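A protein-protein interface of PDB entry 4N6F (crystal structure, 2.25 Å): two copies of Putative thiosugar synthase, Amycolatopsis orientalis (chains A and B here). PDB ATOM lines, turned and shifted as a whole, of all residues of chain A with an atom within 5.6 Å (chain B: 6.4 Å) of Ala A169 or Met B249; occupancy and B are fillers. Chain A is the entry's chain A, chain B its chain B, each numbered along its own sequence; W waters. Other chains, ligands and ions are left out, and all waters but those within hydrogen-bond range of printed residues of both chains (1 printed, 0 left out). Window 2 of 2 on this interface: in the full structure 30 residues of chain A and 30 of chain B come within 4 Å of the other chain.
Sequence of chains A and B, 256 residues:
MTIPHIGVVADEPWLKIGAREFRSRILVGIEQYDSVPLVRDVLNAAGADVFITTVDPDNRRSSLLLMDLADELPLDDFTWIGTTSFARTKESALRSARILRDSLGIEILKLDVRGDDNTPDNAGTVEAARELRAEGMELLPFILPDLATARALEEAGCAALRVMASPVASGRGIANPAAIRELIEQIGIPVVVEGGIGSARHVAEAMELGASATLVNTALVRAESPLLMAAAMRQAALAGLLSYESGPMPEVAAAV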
ATOM      1  N   PRO A 167      27.033  -0.317  11.924  1.00  0.00           N
ATOM      2  CA  PRO A 167      26.736  -0.159  10.505  1.00  0.00           C
ATOM      3  C   PRO A 167      25.776   0.980  10.194  1.00  0.00           C
ATOM      4  O   PRO A 167      24.886   1.291  10.991  1.00  0.00           O
ATOM      5  CB  PRO A 167      26.127  -1.517  10.114  1.00  0.00           C
ATOM      6  CG  PRO A 167      26.716  -2.478  11.092  1.00  0.00           C
ATOM      7  CD  PRO A 167      26.797  -1.703  12.379  1.00  0.00           C
ATOM      8  N   VAL A 168      25.989   1.585   9.032  1.00  0.00           N
ATOM      9  CA  VAL A 168      25.208   2.719   8.576  1.00  0.00           C
ATOM     10  C   VAL A 168      23.734   2.358   8.495  1.00  0.00           C
ATOM     11  O   VAL A 168      23.379   1.307   7.972  1.00  0.00           O
ATOM     12  CB  VAL A 168      25.704   3.209   7.202  1.00  0.00           C
ATOM     13  CG1 VAL A 168      24.769   4.256   6.610  1.00  0.00           C
ATOM     14  CG2 VAL A 168      27.095   3.795   7.343  1.00  0.00           C
ATOM     15  N   ALA A 169      22.891   3.245   9.025  1.00  0.00           N
ATOM     16  CA  ALA A 169      21.424   3.112   8.993  1.00  0.00           C
ATOM     17  C   ALA A 169      20.889   2.050   9.923  1.00  0.00           C
ATOM     18  O   ALA A 169      19.693   1.780   9.918  1.00  0.00           O
ATOM     19  CB  ALA A 169      20.900   2.885   7.570  1.00  0.00           C
ATOM     20  N   SER A 170      21.745   1.494  10.774  1.00  0.00           N
ATOM     21  CA  SER A 170      21.356   0.349  11.579  1.00  0.00           C
ATOM     22  C   SER A 170      20.763   0.714  12.927  1.00  0.00           C
ATOM     23  O   SER A 170      20.114  -0.122  13.553  1.00  0.00           O
ATOM     24  CB  SER A 170      22.560  -0.571  11.788  1.00  0.00           C
ATOM     25  OG  SER A 170      23.439  -0.049  12.763  1.00  0.00           O
ATOM     26  N   GLY A 171      21.022   1.934  13.410  1.00  0.00           N
ATOM     27  CA  GLY A 171      20.513   2.369  14.711  1.00  0.00           C
ATOM     28  C   GLY A 171      21.006   1.568  15.912  1.00  0.00           C
ATOM     29  O   GLY A 171      20.414   1.638  16.998  1.00  0.00           O
ATOM     30  N   GLY A 195      27.939   6.626  12.235  1.00  0.00           N
ATOM     31  CA  GLY A 195      27.464   5.361  11.700  1.00  0.00           C
ATOM     32  C   GLY A 195      26.673   4.569  12.720  1.00  0.00           C
ATOM     33  O   GLY A 195      27.204   4.141  13.749  1.00  0.00           O
ATOM     34  N   GLY A 196      25.393   4.369  12.432  1.00  0.00           N
ATOM     35  CA  GLY A 196      24.553   3.521  13.266  1.00  0.00           C
ATOM     36  C   GLY A 196      24.032   4.187  14.527  1.00  0.00           C
ATOM     37  O   GLY A 196      23.444   3.522  15.371  1.00  0.00           O
ATOM     38  N   ILE A 197      24.241   5.497  14.658  1.00  0.00           N
ATOM     39  CA  ILE A 197      23.663   6.243  15.758  1.00  0.00           C
ATOM     40  C   ILE A 197      22.142   6.232  15.588  1.00  0.00           C
ATOM     41  O   ILE A 197      21.610   6.526  14.511  1.00  0.00           O
ATOM     42  CB  ILE A 197      24.159   7.702  15.827  1.00  0.00           C
ATOM     43  CG1 ILE A 197      25.678   7.762  16.020  1.00  0.00           C
ATOM     44  CG2 ILE A 197      23.460   8.445  16.961  1.00  0.00           C
ATOM     45  CD1 ILE A 197      26.169   7.136  17.306  1.00  0.00           C
ATOM     46  N   GLY A 198      21.467   5.911  16.678  1.00  0.00           N
ATOM     47  CA  GLY A 198      20.035   5.637  16.692  1.00  0.00           C
ATOM     48  C   GLY A 198      19.239   6.640  17.503  1.00  0.00           C
ATOM     49  O   GLY A 198      18.112   6.979  17.132  1.00  0.00           O
ATOM     50  N   THR A 218      20.543   8.920   9.717  1.00  0.00           N
ATOM     51  CA  THR A 218      19.382   8.065   9.730  1.00  0.00           C
ATOM     52  C   THR A 218      18.499   8.218  10.974  1.00  0.00           C
ATOM     53  O   THR A 218      17.328   8.151  10.874  1.00  0.00           O
ATOM     54  CB  THR A 218      19.771   6.585   9.559  1.00  0.00           C
ATOM     55  OG1 THR A 218      20.384   6.401   8.312  1.00  0.00           O
ATOM     56  CG2 THR A 218      18.589   5.707   9.621  1.00  0.00           C
ATOM     57  N   ALA A 219      19.081   8.409  12.136  1.00  0.00           N
ATOM     58  CA  ALA A 219      18.317   8.593  13.382  1.00  0.00           C
ATOM     59  C   ALA A 219      17.307   9.747  13.350  1.00  0.00           C
ATOM     60  O   ALA A 219      16.261   9.684  14.010  1.00  0.00           O
ATOM     61  CB  ALA A 219      19.261   8.794  14.551  1.00  0.00           C
ATOM     62  N   ARG A 222      14.513   8.898  10.335  1.00  0.00           N
ATOM     63  CA  ARG A 222      13.582   7.816  10.663  1.00  0.00           C
ATOM     64  C   ARG A 222      12.881   7.971  11.996  1.00  0.00           C
ATOM     65  O   ARG A 222      12.159   7.074  12.400  1.00  0.00           O
ATOM     66  CB  ARG A 222      14.275   6.444  10.620  1.00  0.00           C
ATOM     67  CG  ARG A 222      14.881   6.091   9.267  1.00  0.00           C
ATOM     68  CD  ARG A 222      14.450   4.720   8.760  1.00  0.00           C
ATOM     69  NE  ARG A 222      15.360   3.627   9.124  1.00  0.00           N
ATOM     70  CZ  ARG A 222      16.300   3.096   8.330  1.00  0.00           C
ATOM     71  NH1 ARG A 222      16.514   3.553   7.094  1.00  0.00           N
ATOM     72  NH2 ARG A 222      17.054   2.096   8.783  1.00  0.00           N
ATOM     73  N   ALA A 223      13.086   9.083  12.694  1.00  0.00           N
ATOM     74  CA  ALA A 223      12.330   9.339  13.922  1.00  0.00           C
ATOM     75  C   ALA A 223      10.942   9.861  13.556  1.00  0.00           C
ATOM     76  O   ALA A 223      10.788  10.519  12.540  1.00  0.00           O
ATOM     77  CB  ALA A 223      13.054  10.341  14.814  1.00  0.00           C
ATOM     78  N   MET A 229      14.148  14.917  17.764  1.00  0.00           N
ATOM     79  CA  MET A 229      15.332  14.070  17.915  1.00  0.00           C
ATOM     80  C   MET A 229      16.604  14.879  17.675  1.00  0.00           C
ATOM     81  O   MET A 229      17.576  14.713  18.390  1.00  0.00           O
ATOM     82  CB  MET A 229      15.300  12.858  16.981  1.00  0.00           C
ATOM     83  CG  MET A 229      16.515  11.938  17.116  1.00  0.00           C
ATOM     84  SD  MET A 229      16.731  11.265  18.770  1.00  0.00           S
ATOM     85  CE  MET A 229      15.693   9.806  18.705  1.00  0.00           C
ATOM     86  N   GLY B 247       9.981   9.618  19.235  1.00  0.00           N
ATOM     87  CA  GLY B 247       9.797   8.343  18.603  1.00  0.00           C
ATOM     88  C   GLY B 247      10.943   7.809  17.792  1.00  0.00           C
ATOM     89  O   GLY B 247      10.914   7.876  16.609  1.00  0.00           O
ATOM     90  N   PRO B 248      11.985   7.346  18.456  1.00  0.00           N
ATOM     91  CA  PRO B 248      13.202   6.901  17.775  1.00  0.00           C
ATOM     92  C   PRO B 248      12.953   5.747  16.805  1.00  0.00           C
ATOM     93  O   PRO B 248      12.011   4.971  16.988  1.00  0.00           O
ATOM     94  CB  PRO B 248      14.109   6.424  18.918  1.00  0.00           C
ATOM     95  CG  PRO B 248      13.465   6.858  20.182  1.00  0.00           C
ATOM     96  CD  PRO B 248      12.016   7.055  19.899  1.00  0.00           C
ATOM     97  N   MET B 249      13.806   5.645  15.789  1.00  0.00           N
ATOM     98  CA  MET B 249      13.774   4.526  14.856  1.00  0.00           C
ATOM     99  C   MET B 249      13.679   3.210  15.635  1.00  0.00           C
ATOM    100  O   MET B 249      14.373   3.046  16.643  1.00  0.00           O
ATOM    101  CB  MET B 249      15.009   4.546  13.946  1.00  0.00           C
ATOM    102  CG  MET B 249      16.350   4.392  14.663  1.00  0.00           C
ATOM    103  SD  MET B 249      17.756   4.682  13.575  1.00  0.00           S
ATOM    104  CE  MET B 249      17.681   3.233  12.520  1.00  0.00           C
ATOM    105  N   PRO B 250      12.940   2.259  15.126  1.00  0.00           N
ATOM    106  CA  PRO B 250      12.475   1.108  15.885  1.00  0.00           C
ATOM    107  C   PRO B 250      13.582   0.255  16.499  1.00  0.00           C
ATOM    108  O   PRO B 250      13.433  -0.261  17.579  1.00  0.00           O
ATOM    109  CB  PRO B 250      11.743   0.299  14.842  1.00  0.00           C
ATOM    110  CG  PRO B 250      11.340   1.263  13.818  1.00  0.00           C
ATOM    111  CD  PRO B 250      12.214   2.447  13.878  1.00  0.00           C
ATOM    112  N   GLU B 251      14.676   0.103  15.801  1.00  0.00           N
ATOM    113  CA  GLU B 251      15.801  -0.752  16.235  1.00  0.00           C
ATOM    114  C   GLU B 251      16.597  -0.195  17.421  1.00  0.00           C
ATOM    115  O   GLU B 251      17.497  -0.868  17.930  1.00  0.00           O
ATOM    116  CB  GLU B 251      16.748  -1.103  15.073  1.00  0.00           C
ATOM    117  CG  GLU B 251      16.974   0.001  14.060  1.00  0.00           C
ATOM    118  CD  GLU B 251      15.890   0.062  12.998  1.00  0.00           C
ATOM    119  OE1 GLU B 251      14.983   0.908  13.140  1.00  0.00           O
ATOM    120  OE2 GLU B 251      15.943  -0.737  12.039  1.00  0.00           O
ATOM    121  N   VAL B 252      16.268   1.021  17.859  1.00  0.00           N
ATOM    122  CA  VAL B 252      16.760   1.541  19.134  1.00  0.00           C
ATOM    123  C   VAL B 252      16.083   0.801  20.298  1.00  0.00           C
ATOM    124  O   VAL B 252      16.729   0.499  21.303  1.00  0.00           O
ATOM    125  CB  VAL B 252      16.531   3.065  19.253  1.00  0.00           C
ATOM    126  CG1 VAL B 252      16.878   3.567  20.648  1.00  0.00           C
ATOM    127  CG2 VAL B 252      17.358   3.802  18.211  1.00  0.00           C
ATOM    128  N   ALA B 253      14.784   0.524  20.159  1.00  0.00           N
ATOM    129  CA  ALA B 253      14.052  -0.320  21.111  1.00  0.00           C
ATOM    130  C   ALA B 253      14.024  -1.769  20.620  1.00  0.00           C
ATOM    131  O   ALA B 253      14.878  -2.578  20.983  1.00  0.00           O
ATOM    132  CB  ALA B 253      12.633   0.201  21.302  1.00  0.00           C
HETATM  133  O   HOH W   1      15.919   7.566  15.574  1.00  0.00           O
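Of the 7 printed residues of chain B, 5 touch a printed residue of chain A.
Hydrophobic or aromatic side chains of chain B within 4 Å of the printed part of chain A: Pro B248, Met B249 and Val B252.
Printed residues of chain A that touch a printed residue of chain B: Ala A169, Ser A170, Gly A171, Gly A198, Thr A218, Ala A219, Arg A222, Ala A223 and Met A229.
Hydrophobic or aromatic side chains of chain A that line the printed part of chain B: Ala A223 and Met A229.
Water W1 lies within hydrogen-bond range of O of Ala A219 (2.7 Å), O of Gly A198 (2.8 Å) and N of Met B249 (2.9 Å).
The side-chain hydroxyl (OG) of Ser A170 is in hydrogen-bond range of the backbone carbonyl oxygen (O) of Pro A167, at 2.7 Å.
O of Ala A169 sits at hydrogen-bond distance from NH2 of Arg A222 (2.9 Å).
N of Gly A171 lies close to O of Gly A196, at 3.5 Å.
Of the printed residues of chain B, Gly A198 touches Met B249 and Val B252.
Of the printed residues of chain B, Thr A218 touches Met B249 (3.9 Å).
Printed residues of chain A within 4 Å of Pro B248: Met A229 (3.7 Å).
The nearest printed residue of chain A that does not touch Met B249 is Ser A170 (4.001 Å).
No position is printed for both chains.
Of the 12 pairs that touch across the chains among the printed residues, none has its exchanged pair printed and touching as well.
Ala A169 touches Met B249 (O to CE, 3.6 Å).
Glu B251 touches Ser A170 (CG to O, 3.2 Å).
CE of Met B249 touches CA of Gly A171 (3.7 Å).
Val B252 touches Gly A171.
CA of Gly A198 touches SD of Met B249, 3.98 Å away.
CE of Met B249 touches CG2 of Thr A218, 3.9 Å away.
SD of Met B249 touches CA of Ala A219, at 3.96 Å.
O of Arg A222 touches CA of Met B249, 3.9 Å away.
Ala A223 touches Gly B247.
Met A229 touches Pro B248.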
